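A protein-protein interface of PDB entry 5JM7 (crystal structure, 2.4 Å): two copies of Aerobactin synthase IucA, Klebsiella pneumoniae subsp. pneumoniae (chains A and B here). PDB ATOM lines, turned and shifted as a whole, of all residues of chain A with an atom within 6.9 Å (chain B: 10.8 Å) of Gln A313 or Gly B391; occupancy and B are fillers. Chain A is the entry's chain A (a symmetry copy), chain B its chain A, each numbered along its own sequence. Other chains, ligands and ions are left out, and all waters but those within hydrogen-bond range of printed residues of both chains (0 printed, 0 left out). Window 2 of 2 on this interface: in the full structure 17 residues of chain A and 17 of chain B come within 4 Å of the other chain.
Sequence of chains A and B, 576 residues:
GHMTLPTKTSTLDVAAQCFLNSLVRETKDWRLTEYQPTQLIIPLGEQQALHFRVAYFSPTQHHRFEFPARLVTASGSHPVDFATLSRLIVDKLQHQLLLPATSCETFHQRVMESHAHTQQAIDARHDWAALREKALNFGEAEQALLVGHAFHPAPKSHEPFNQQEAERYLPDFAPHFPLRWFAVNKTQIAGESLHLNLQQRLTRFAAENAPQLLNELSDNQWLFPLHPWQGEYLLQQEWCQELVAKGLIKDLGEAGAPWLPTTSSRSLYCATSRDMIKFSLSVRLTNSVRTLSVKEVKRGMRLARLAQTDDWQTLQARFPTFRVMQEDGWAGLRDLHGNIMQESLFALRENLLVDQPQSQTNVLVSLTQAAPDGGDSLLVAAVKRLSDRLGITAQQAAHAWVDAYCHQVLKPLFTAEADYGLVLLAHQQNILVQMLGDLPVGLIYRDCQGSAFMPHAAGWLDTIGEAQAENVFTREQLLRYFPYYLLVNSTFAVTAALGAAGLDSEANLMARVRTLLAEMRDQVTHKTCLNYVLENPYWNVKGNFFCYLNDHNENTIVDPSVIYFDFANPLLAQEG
NH2 of Arg A323 is in hydrogen-bond range of O of Arg B389 (3.2 Å).
The side-chain amide nitrogen of Gln A313 is in hydrogen-bond range of the backbone carbonyl oxygen of Gly B391, at 3.2 Å.
The side-chain hydroxyl of Ser B387 lies within hydrogen-bond range of the backbone carbonyl oxygen of Ile B392 (2.5 Å).
The guanidinium group (NH2) of Arg B389 lies within hydrogen-bond range of the backbone carbonyl oxygen (O) of Gly B437 (2.9 Å).
N of Gln B396 lies within hydrogen-bond range of OG1 of Thr B393 (3.0 Å).
O of Asp A310 sits at hydrogen-bond distance from OG1 of Thr A314 (3.0 Å).
The side-chain amide oxygen (OE1) of Gln A316 is in hydrogen-bond range of the guanidinium group (NH1) of Arg A323.
Among the printed residues, merely in contact across the chains: Gln A313 with Ile B392, Gln A313 with Thr B393, Gln A313 with Gln B396, Thr A314 with Gln B396, Gln A316 with Leu B390, Gln A316 with Ile B392, Ala A317 with Ile B392, Ala A317 with Gln B396 and Arg A323 with Leu B390.
Asp A310 touches none of the printed residues of chain B.
Gln A313 touches just these residues of chain B: Gly B391, Ile B392, Thr B393 and Gln B396.
Of the printed residues of chain B, Thr A314 touches Gln B396.
Of chain B, only Ile B392 and Gln B396 come within 4 Å of Ala A317.
Printed residues of chain A within 4 Å of Arg B389: Arg A323 (3.2 Å).
Gly B391 touches just one residue of chain A: Gln A313 (3.2 Å).
The nearest residue of chain B that does not touch Gln A313 is Leu B390 (5.9 Å).
Of the 16 printed residues of chain A, 5 touch a printed residue of chain B.
Printed residues of chain A that touch a printed residue of chain B: Gln A313, Thr A314, Gln A316, Ala A317 and Arg A323.
Hydrophobic or aromatic side chains of chain A that line the printed part of chain B: Ala A317.
No position is printed for both chains.
Of the 11 pairs that touch across the chains among the printed residues, none has its exchanged pair printed and touching as well.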
ATOM      1  N   LEU A 306      -5.202   7.940   1.678  1.00  0.00           N
ATOM      2  CA  LEU A 306      -4.683   6.874   2.518  1.00  0.00           C
ATOM      3  C   LEU A 306      -3.201   7.091   2.798  1.00  0.00           C
ATOM      4  O   LEU A 306      -2.711   6.735   3.883  1.00  0.00           O
ATOM      5  CB  LEU A 306      -4.916   5.518   1.853  1.00  0.00           C
ATOM      6  CG  LEU A 306      -4.537   4.364   2.755  1.00  0.00           C
ATOM      7  CD1 LEU A 306      -5.506   4.378   3.940  1.00  0.00           C
ATOM      8  CD2 LEU A 306      -4.598   3.044   1.992  1.00  0.00           C
ATOM      9  N   ALA A 307      -2.476   7.703   1.842  1.00  0.00           N
ATOM     10  CA  ALA A 307      -1.057   7.971   2.039  1.00  0.00           C
ATOM     11  C   ALA A 307      -0.782   9.063   3.074  1.00  0.00           C
ATOM     12  O   ALA A 307       0.389   9.270   3.421  1.00  0.00           O
ATOM     13  CB  ALA A 307      -0.375   8.313   0.710  1.00  0.00           C
ATOM     14  N   GLN A 308      -1.805   9.716   3.624  1.00  0.00           N
ATOM     15  CA  GLN A 308      -1.595  10.673   4.706  1.00  0.00           C
ATOM     16  C   GLN A 308      -1.640  10.033   6.093  1.00  0.00           C
ATOM     17  O   GLN A 308      -1.386  10.738   7.082  1.00  0.00           O
ATOM     18  CB  GLN A 308      -2.646  11.782   4.677  1.00  0.00           C
ATOM     19  CG  GLN A 308      -2.710  12.563   3.396  1.00  0.00           C
ATOM     20  CD  GLN A 308      -1.386  13.236   3.053  1.00  0.00           C
ATOM     21  OE1 GLN A 308      -0.965  14.169   3.735  1.00  0.00           O
ATOM     22  NE2 GLN A 308      -0.782  12.833   1.940  1.00  0.00           N
ATOM     23  N   THR A 309      -1.958   8.737   6.204  1.00  0.00           N
ATOM     24  CA  THR A 309      -2.220   8.163   7.515  1.00  0.00           C
ATOM     25  C   THR A 309      -0.916   7.755   8.193  1.00  0.00           C
ATOM     26  O   THR A 309       0.169   7.842   7.617  1.00  0.00           O
ATOM     27  CB  THR A 309      -3.173   6.972   7.401  1.00  0.00           C
ATOM     28  OG1 THR A 309      -2.572   5.948   6.599  1.00  0.00           O
ATOM     29  CG2 THR A 309      -4.460   7.396   6.720  1.00  0.00           C
ATOM     30  N   ASP A 310      -1.022   7.337   9.453  1.00  0.00           N
ATOM     31  CA  ASP A 310       0.182   6.957  10.195  1.00  0.00           C
ATOM     32  C   ASP A 310       0.724   5.602   9.748  1.00  0.00           C
ATOM     33  O   ASP A 310       1.939   5.373   9.814  1.00  0.00           O
ATOM     34  CB  ASP A 310      -0.081   6.900  11.699  1.00  0.00           C
ATOM     35  CG  ASP A 310      -0.337   8.257  12.310  1.00  0.00           C
ATOM     36  OD1 ASP A 310      -0.125   9.283  11.643  1.00  0.00           O
ATOM     37  OD2 ASP A 310      -0.708   8.295  13.494  1.00  0.00           O
ATOM     38  N   ASP A 311      -0.154   4.686   9.327  1.00  0.00           N
ATOM     39  CA  ASP A 311       0.326   3.395   8.850  1.00  0.00           C
ATOM     40  C   ASP A 311       0.995   3.520   7.491  1.00  0.00           C
ATOM     41  O   ASP A 311       1.977   2.815   7.219  1.00  0.00           O
ATOM     42  CB  ASP A 311      -0.805   2.380   8.774  1.00  0.00           C
ATOM     43  CG  ASP A 311      -1.233   1.894  10.135  1.00  0.00           C
ATOM     44  OD1 ASP A 311      -0.500   2.152  11.120  1.00  0.00           O
ATOM     45  OD2 ASP A 311      -2.271   1.209  10.203  1.00  0.00           O
ATOM     46  N   TRP A 312       0.493   4.401   6.626  1.00  0.00           N
ATOM     47  CA  TRP A 312       1.219   4.661   5.393  1.00  0.00           C
ATOM     48  C   TRP A 312       2.613   5.179   5.727  1.00  0.00           C
ATOM     49  O   TRP A 312       3.613   4.742   5.150  1.00  0.00           O
ATOM     50  CB  TRP A 312       0.504   5.688   4.523  1.00  0.00           C
ATOM     51  CG  TRP A 312       1.228   5.809   3.215  1.00  0.00           C
ATOM     52  CD1 TRP A 312       2.307   6.607   2.946  1.00  0.00           C
ATOM     53  CD2 TRP A 312       0.841   5.223   1.961  1.00  0.00           C
ATOM     54  NE1 TRP A 312       2.680   6.460   1.637  1.00  0.00           N
ATOM     55  CE2 TRP A 312       1.791   5.634   1.004  1.00  0.00           C
ATOM     56  CE3 TRP A 312      -0.206   4.376   1.566  1.00  0.00           C
ATOM     57  CZ2 TRP A 312       1.724   5.246  -0.324  1.00  0.00           C
ATOM     58  CZ3 TRP A 312      -0.266   3.974   0.256  1.00  0.00           C
ATOM     59  CH2 TRP A 312       0.693   4.414  -0.684  1.00  0.00           C
ATOM     60  N   GLN A 313       2.682   6.064   6.701  1.00  0.00           N
ATOM     61  CA  GLN A 313       3.929   6.636   7.124  1.00  0.00           C
ATOM     62  C   GLN A 313       4.861   5.559   7.637  1.00  0.00           C
ATOM     63  O   GLN A 313       6.006   5.539   7.279  1.00  0.00           O
ATOM     64  CB  GLN A 313       3.650   7.662   8.202  1.00  0.00           C
ATOM     65  CG  GLN A 313       4.668   8.746   8.379  1.00  0.00           C
ATOM     66  CD  GLN A 313       4.345   9.623   9.552  1.00  0.00           C
ATOM     67  OE1 GLN A 313       3.725   9.201  10.485  1.00  0.00           O
ATOM     68  NE2 GLN A 313       4.769  10.837   9.502  1.00  0.00           N
ATOM     69  N   THR A 314       4.359   4.645   8.447  1.00  0.00           N
ATOM     70  CA  THR A 314       5.163   3.531   8.956  1.00  0.00           C
ATOM     71  C   THR A 314       5.716   2.677   7.816  1.00  0.00           C
ATOM     72  O   THR A 314       6.880   2.255   7.851  1.00  0.00           O
ATOM     73  CB  THR A 314       4.325   2.670   9.920  1.00  0.00           C
ATOM     74  OG1 THR A 314       3.938   3.452  11.053  1.00  0.00           O
ATOM     75  CG2 THR A 314       5.107   1.460  10.409  1.00  0.00           C
ATOM     76  N   LEU A 315       4.883   2.405   6.807  1.00  0.00           N
ATOM     77  CA  LEU A 315       5.318   1.666   5.626  1.00  0.00           C
ATOM     78  C   LEU A 315       6.416   2.410   4.873  1.00  0.00           C
ATOM     79  O   LEU A 315       7.425   1.814   4.464  1.00  0.00           O
ATOM     80  CB  LEU A 315       4.120   1.428   4.708  1.00  0.00           C
ATOM     81  CG  LEU A 315       4.418   0.833   3.333  1.00  0.00           C
ATOM     82  CD1 LEU A 315       5.013  -0.545   3.454  1.00  0.00           C
ATOM     83  CD2 LEU A 315       3.147   0.803   2.505  1.00  0.00           C
ATOM     84  N   GLN A 316       6.212   3.714   4.643  1.00  0.00           N
ATOM     85  CA  GLN A 316       7.220   4.509   3.963  1.00  0.00           C
ATOM     86  C   GLN A 316       8.521   4.492   4.743  1.00  0.00           C
ATOM     87  O   GLN A 316       9.599   4.364   4.155  1.00  0.00           O
ATOM     88  CB  GLN A 316       6.725   5.947   3.759  1.00  0.00           C
ATOM     89  CG  GLN A 316       7.746   6.817   3.029  1.00  0.00           C
ATOM     90  CD  GLN A 316       7.912   6.436   1.573  1.00  0.00           C
ATOM     91  OE1 GLN A 316       7.039   6.703   0.735  1.00  0.00           O
ATOM     92  NE2 GLN A 316       8.975   5.688   1.289  1.00  0.00           N
ATOM     93  N   ALA A 317       8.441   4.586   6.078  1.00  0.00           N
ATOM     94  CA  ALA A 317       9.658   4.604   6.893  1.00  0.00           C
ATOM     95  C   ALA A 317      10.405   3.283   6.813  1.00  0.00           C
ATOM     96  O   ALA A 317      11.640   3.259   6.936  1.00  0.00           O
ATOM     97  CB  ALA A 317       9.330   4.928   8.349  1.00  0.00           C
ATOM     98  N   ARG A 318       9.676   2.179   6.584  1.00  0.00           N
ATOM     99  CA  ARG A 318      10.287   0.859   6.449  1.00  0.00           C
ATOM    100  C   ARG A 318      10.945   0.669   5.081  1.00  0.00           C
ATOM    101  O   ARG A 318      11.930  -0.067   4.969  1.00  0.00           O
ATOM    102  CB  ARG A 318       9.226  -0.220   6.690  1.00  0.00           C
ATOM    103  CG  ARG A 318       9.712  -1.641   6.625  1.00  0.00           C
ATOM    104  CD  ARG A 318       8.565  -2.634   6.875  1.00  0.00           C
ATOM    105  NE  ARG A 318       9.008  -4.020   6.770  1.00  0.00           N
ATOM    106  CZ  ARG A 318       8.229  -5.069   6.993  1.00  0.00           C
ATOM    107  NH1 ARG A 318       6.955  -4.899   7.312  1.00  0.00           N
ATOM    108  NH2 ARG A 318       8.710  -6.291   6.839  1.00  0.00           N
ATOM    109  N   ARG A 323       8.656   4.452  -3.436  1.00  0.00           N
ATOM    110  CA  ARG A 323       7.812   5.634  -3.559  1.00  0.00           C
ATOM    111  C   ARG A 323       6.642   5.340  -4.485  1.00  0.00           C
ATOM    112  O   ARG A 323       6.785   4.621  -5.479  1.00  0.00           O
ATOM    113  CB  ARG A 323       8.612   6.849  -4.106  1.00  0.00           C
ATOM    114  CG  ARG A 323       9.731   7.312  -3.186  1.00  0.00           C
ATOM    115  CD  ARG A 323       9.157   8.066  -2.008  1.00  0.00           C
ATOM    116  NE  ARG A 323       8.940   9.474  -2.341  1.00  0.00           N
ATOM    117  CZ  ARG A 323       8.039  10.251  -1.755  1.00  0.00           C
ATOM    118  NH1 ARG A 323       7.246   9.751  -0.810  1.00  0.00           N
ATOM    119  NH2 ARG A 323       7.933  11.521  -2.127  1.00  0.00           N
ATOM    120  N   TYR A 420       0.079  -4.902   5.082  1.00  0.00           N
ATOM    121  CA  TYR A 420      -0.793  -3.733   5.047  1.00  0.00           C
ATOM    122  C   TYR A 420      -2.076  -3.945   4.254  1.00  0.00           C
ATOM    123  O   TYR A 420      -3.002  -3.138   4.382  1.00  0.00           O
ATOM    124  CB  TYR A 420      -0.020  -2.520   4.480  1.00  0.00           C
ATOM    125  CG  TYR A 420       1.043  -2.009   5.429  1.00  0.00           C
ATOM    126  CD1 TYR A 420       2.286  -2.639   5.521  1.00  0.00           C
ATOM    127  CD2 TYR A 420       0.776  -0.949   6.305  1.00  0.00           C
ATOM    128  CE1 TYR A 420       3.253  -2.200   6.415  1.00  0.00           C
ATOM    129  CE2 TYR A 420       1.738  -0.511   7.202  1.00  0.00           C
ATOM    130  CZ  TYR A 420       2.971  -1.145   7.257  1.00  0.00           C
ATOM    131  OH  TYR A 420       3.917  -0.709   8.153  1.00  0.00           O
ATOM    132  N   TRP A 460      -7.894  -0.214   8.346  1.00  0.00           N
ATOM    133  CA  TRP A 460      -7.100   0.948   7.971  1.00  0.00           C
ATOM    134  C   TRP A 460      -7.808   1.811   6.924  1.00  0.00           C
ATOM    135  O   TRP A 460      -7.789   3.042   7.031  1.00  0.00           O
ATOM    136  CB  TRP A 460      -5.695   0.463   7.576  1.00  0.00           C
ATOM    137  CG  TRP A 460      -4.710   1.448   6.980  1.00  0.00           C
ATOM    138  CD1 TRP A 460      -4.183   2.559   7.590  1.00  0.00           C
ATOM    139  CD2 TRP A 460      -3.887   1.220   5.813  1.00  0.00           C
ATOM    140  NE1 TRP A 460      -3.218   3.126   6.791  1.00  0.00           N
ATOM    141  CE2 TRP A 460      -2.996   2.311   5.711  1.00  0.00           C
ATOM    142  CE3 TRP A 460      -3.852   0.224   4.826  1.00  0.00           C
ATOM    143  CZ2 TRP A 460      -2.092   2.440   4.655  1.00  0.00           C
ATOM    144  CZ3 TRP A 460      -2.955   0.353   3.778  1.00  0.00           C
ATOM    145  CH2 TRP A 460      -2.085   1.452   3.698  1.00  0.00           C
ATOM    146  N   ALA B 382      20.596  16.587   6.751  1.00  0.00           N
ATOM    147  CA  ALA B 382      20.257  15.598   5.727  1.00  0.00           C
ATOM    148  C   ALA B 382      19.058  14.738   6.149  1.00  0.00           C
ATOM    149  O   ALA B 382      18.142  14.504   5.343  1.00  0.00           O
ATOM    150  CB  ALA B 382      21.471  14.714   5.427  1.00  0.00           C
ATOM    151  N   VAL B 383      19.042  14.270   7.412  1.00  0.00           N
ATOM    152  CA  VAL B 383      17.936  13.449   7.906  1.00  0.00           C
ATOM    153  C   VAL B 383      16.624  14.236   7.927  1.00  0.00           C
ATOM    154  O   VAL B 383      15.566  13.702   7.559  1.00  0.00           O
ATOM    155  CB  VAL B 383      18.266  12.865   9.296  1.00  0.00           C
ATOM    156  CG1 VAL B 383      17.050  12.146   9.851  1.00  0.00           C
ATOM    157  CG2 VAL B 383      19.465  11.929   9.213  1.00  0.00           C
ATOM    158  N   LYS B 384      16.658  15.510   8.351  1.00  0.00           N
ATOM    159  CA  LYS B 384      15.429  16.313   8.313  1.00  0.00           C
ATOM    160  C   LYS B 384      14.893  16.481   6.895  1.00  0.00           C
ATOM    161  O   LYS B 384      13.677  16.409   6.684  1.00  0.00           O
ATOM    162  CB  LYS B 384      15.630  17.666   8.983  1.00  0.00           C
ATOM    163  CG  LYS B 384      15.743  17.484  10.508  1.00  0.00           C
ATOM    164  CD  LYS B 384      16.002  18.797  11.199  1.00  0.00           C
ATOM    165  CE  LYS B 384      16.034  18.557  12.682  1.00  0.00           C
ATOM    166  NZ  LYS B 384      16.359  19.772  13.465  1.00  0.00           N
ATOM    167  N   ARG B 385      15.776  16.670   5.901  1.00  0.00           N
ATOM    168  CA  ARG B 385      15.311  16.667   4.513  1.00  0.00           C
ATOM    169  C   ARG B 385      14.738  15.310   4.131  1.00  0.00           C
ATOM    170  O   ARG B 385      13.754  15.238   3.393  1.00  0.00           O
ATOM    171  CB  ARG B 385      16.440  17.047   3.557  1.00  0.00           C
ATOM    172  CG  ARG B 385      16.911  18.528   3.604  1.00  0.00           C
ATOM    173  CD  ARG B 385      17.846  18.811   2.418  1.00  0.00           C
ATOM    174  NE  ARG B 385      19.062  17.992   2.464  1.00  0.00           N
ATOM    175  CZ  ARG B 385      20.180  18.328   3.108  1.00  0.00           C
ATOM    176  NH1 ARG B 385      20.259  19.503   3.732  1.00  0.00           N
ATOM    177  NH2 ARG B 385      21.222  17.492   3.111  1.00  0.00           N
ATOM    178  N   LEU B 386      15.357  14.222   4.603  1.00  0.00           N
ATOM    179  CA  LEU B 386      14.819  12.891   4.329  1.00  0.00           C
ATOM    180  C   LEU B 386      13.397  12.775   4.882  1.00  0.00           C
ATOM    181  O   LEU B 386      12.462  12.387   4.172  1.00  0.00           O
ATOM    182  CB  LEU B 386      15.739  11.813   4.938  1.00  0.00           C
ATOM    183  CG  LEU B 386      15.332  10.352   4.737  1.00  0.00           C
ATOM    184  CD1 LEU B 386      15.336   9.997   3.255  1.00  0.00           C
ATOM    185  CD2 LEU B 386      16.220   9.392   5.511  1.00  0.00           C
ATOM    186  N   SER B 387      13.228  13.130   6.157  1.00  0.00           N
ATOM    187  CA  SER B 387      11.923  13.256   6.800  1.00  0.00           C
ATOM    188  C   SER B 387      10.911  14.010   5.930  1.00  0.00           C
ATOM    189  O   SER B 387       9.804  13.516   5.688  1.00  0.00           O
ATOM    190  CB  SER B 387      12.124  13.962   8.145  1.00  0.00           C
ATOM    191  OG  SER B 387      10.905  14.215   8.805  1.00  0.00           O
ATOM    192  N   ASP B 388      11.276  15.219   5.455  1.00  0.00           N
ATOM    193  CA  ASP B 388      10.333  16.048   4.697  1.00  0.00           C
ATOM    194  C   ASP B 388       9.972  15.420   3.356  1.00  0.00           C
ATOM    195  O   ASP B 388       8.796  15.397   2.966  1.00  0.00           O
ATOM    196  CB  ASP B 388      10.904  17.442   4.463  1.00  0.00           C
ATOM    197  CG  ASP B 388      10.968  18.250   5.738  1.00  0.00           C
ATOM    198  OD1 ASP B 388      10.332  17.844   6.745  1.00  0.00           O
ATOM    199  OD2 ASP B 388      11.667  19.280   5.734  1.00  0.00           O
ATOM    200  N   ARG B 389      10.977  14.947   2.603  1.00  0.00           N
ATOM    201  CA  ARG B 389      10.719  14.422   1.262  1.00  0.00           C
ATOM    202  C   ARG B 389       9.808  13.193   1.310  1.00  0.00           C
ATOM    203  O   ARG B 389       8.916  13.040   0.465  1.00  0.00           O
ATOM    204  CB  ARG B 389      12.050  14.109   0.575  1.00  0.00           C
ATOM    205  CG  ARG B 389      11.941  13.512  -0.827  1.00  0.00           C
ATOM    206  CD  ARG B 389      13.306  13.323  -1.493  1.00  0.00           C
ATOM    207  NE  ARG B 389      14.169  12.364  -0.808  1.00  0.00           N
ATOM    208  CZ  ARG B 389      14.105  11.042  -0.968  1.00  0.00           C
ATOM    209  NH1 ARG B 389      13.202  10.520  -1.782  1.00  0.00           N
ATOM    210  NH2 ARG B 389      14.935  10.242  -0.313  1.00  0.00           N
ATOM    211  N   LEU B 390      10.002  12.318   2.304  1.00  0.00           N
ATOM    212  CA  LEU B 390       9.232  11.080   2.409  1.00  0.00           C
ATOM    213  C   LEU B 390       7.957  11.227   3.237  1.00  0.00           C
ATOM    214  O   LEU B 390       7.131  10.314   3.232  1.00  0.00           O
ATOM    215  CB  LEU B 390      10.093   9.963   3.012  1.00  0.00           C
ATOM    216  CG  LEU B 390      11.329   9.462   2.261  1.00  0.00           C
ATOM    217  CD1 LEU B 390      12.055   8.416   3.106  1.00  0.00           C
ATOM    218  CD2 LEU B 390      11.005   8.923   0.854  1.00  0.00           C
ATOM    219  N   GLY B 391       7.775  12.345   3.935  1.00  0.00           N
ATOM    220  CA  GLY B 391       6.597  12.495   4.770  1.00  0.00           C
ATOM    221  C   GLY B 391       6.609  11.607   5.997  1.00  0.00           C
ATOM    222  O   GLY B 391       5.551  11.134   6.428  1.00  0.00           O
ATOM    223  N   ILE B 392       7.783  11.348   6.567  1.00  0.00           N
ATOM    224  CA  ILE B 392       7.910  10.527   7.760  1.00  0.00           C
ATOM    225  C   ILE B 392       8.507  11.385   8.869  1.00  0.00           C
ATOM    226  O   ILE B 392       9.125  12.416   8.615  1.00  0.00           O
ATOM    227  CB  ILE B 392       8.770   9.272   7.494  1.00  0.00           C
ATOM    228  CG1 ILE B 392      10.196   9.658   7.103  1.00  0.00           C
ATOM    229  CG2 ILE B 392       8.144   8.418   6.394  1.00  0.00           C
ATOM    230  CD1 ILE B 392      11.133   8.492   6.992  1.00  0.00           C
ATOM    231  N   THR B 393       8.313  10.955  10.115  1.00  0.00           N
ATOM    232  CA  THR B 393       8.795  11.755  11.230  1.00  0.00           C
ATOM    233  C   THR B 393      10.315  11.838  11.207  1.00  0.00           C
ATOM    234  O   THR B 393      11.008  10.982  10.635  1.00  0.00           O
ATOM    235  CB  THR B 393       8.376  11.174  12.587  1.00  0.00           C
ATOM    236  OG1 THR B 393       8.973   9.877  12.756  1.00  0.00           O
ATOM    237  CG2 THR B 393       6.839  11.078  12.725  1.00  0.00           C
ATOM    238  N   ALA B 394      10.825  12.884  11.866  1.00  0.00           N
ATOM    239  CA  ALA B 394      12.255  13.016  12.103  1.00  0.00           C
ATOM    240  C   ALA B 394      12.845  11.725  12.654  1.00  0.00           C
ATOM    241  O   ALA B 394      13.876  11.245  12.168  1.00  0.00           O
ATOM    242  CB  ALA B 394      12.519  14.181  13.059  1.00  0.00           C
ATOM    243  N   GLN B 395      12.196  11.132  13.661  1.00  0.00           N
ATOM    244  CA  GLN B 395      12.745   9.911  14.252  1.00  0.00           C
ATOM    245  C   GLN B 395      12.721   8.743  13.267  1.00  0.00           C
ATOM    246  O   GLN B 395      13.668   7.941  13.209  1.00  0.00           O
ATOM    247  CB  GLN B 395      11.997   9.549  15.540  1.00  0.00           C
ATOM    248  CG  GLN B 395      12.565   8.282  16.200  1.00  0.00           C
ATOM    249  CD  GLN B 395      12.004   7.980  17.585  1.00  0.00           C
ATOM    250  OE1 GLN B 395      11.340   8.791  18.202  1.00  0.00           O
ATOM    251  NE2 GLN B 395      12.231   6.783  18.039  1.00  0.00           N
ATOM    252  N   GLN B 396      11.658   8.634  12.476  1.00  0.00           N
ATOM    253  CA  GLN B 396      11.611   7.566  11.479  1.00  0.00           C
ATOM    254  C   GLN B 396      12.678   7.754  10.406  1.00  0.00           C
ATOM    255  O   GLN B 396      13.227   6.776   9.891  1.00  0.00           O
ATOM    256  CB  GLN B 396      10.218   7.491  10.851  1.00  0.00           C
ATOM    257  CG  GLN B 396       9.156   6.929  11.761  1.00  0.00           C
ATOM    258  CD  GLN B 396       7.764   7.063  11.165  1.00  0.00           C
ATOM    259  OE1 GLN B 396       7.491   8.006  10.389  1.00  0.00           O
ATOM    260  NE2 GLN B 396       6.889   6.113  11.492  1.00  0.00           N
ATOM    261  N   ALA B 397      12.984   8.999  10.054  1.00  0.00           N
ATOM    262  CA  ALA B 397      14.076   9.219   9.118  1.00  0.00           C
ATOM    263  C   ALA B 397      15.413   8.874   9.760  1.00  0.00           C
ATOM    264  O   ALA B 397      16.281   8.271   9.113  1.00  0.00           O
ATOM    265  CB  ALA B 397      14.066  10.659   8.607  1.00  0.00           C
ATOM    266  N   ALA B 398      15.604   9.249  11.027  1.00  0.00           N
ATOM    267  CA  ALA B 398      16.831   8.880  11.723  1.00  0.00           C
ATOM    268  C   ALA B 398      17.020   7.369  11.732  1.00  0.00           C
ATOM    269  O   ALA B 398      18.141   6.887  11.520  1.00  0.00           O
ATOM    270  CB  ALA B 398      16.827   9.419  13.153  1.00  0.00           C
ATOM    271  N   HIS B 399      15.932   6.600  11.951  1.00  0.00           N
ATOM    272  CA  HIS B 399      16.037   5.137  11.932  1.00  0.00           C
ATOM    273  C   HIS B 399      16.382   4.627  10.540  1.00  0.00           C
ATOM    274  O   HIS B 399      17.224   3.737  10.390  1.00  0.00           O
ATOM    275  CB  HIS B 399      14.736   4.477  12.402  1.00  0.00           C
ATOM    276  CG  HIS B 399      14.403   4.716  13.846  1.00  0.00           C
ATOM    277  ND1 HIS B 399      13.155   4.444  14.377  1.00  0.00           N
ATOM    278  CD2 HIS B 399      15.161   5.171  14.876  1.00  0.00           C
ATOM    279  CE1 HIS B 399      13.164   4.734  15.669  1.00  0.00           C
ATOM    280  NE2 HIS B 399      14.368   5.176  15.997  1.00  0.00           N
ATOM    281  N   ALA B 400      15.741   5.183   9.512  1.00  0.00           N
ATOM    282  CA  ALA B 400      16.018   4.749   8.147  1.00  0.00           C
ATOM    283  C   ALA B 400      17.473   5.007   7.762  1.00  0.00           C
ATOM    284  O   ALA B 400      18.077   4.204   7.041  1.00  0.00           O
ATOM    285  CB  ALA B 400      15.078   5.445   7.175  1.00  0.00           C
ATOM    286  N   GLY B 437      19.238  11.328  -2.356  1.00  0.00           N
ATOM    287  CA  GLY B 437      18.163  11.939  -1.598  1.00  0.00           C
ATOM    288  C   GLY B 437      18.333  11.808  -0.102  1.00  0.00           C
ATOM    289  O   GLY B 437      17.359  11.502   0.610  1.00  0.00           O
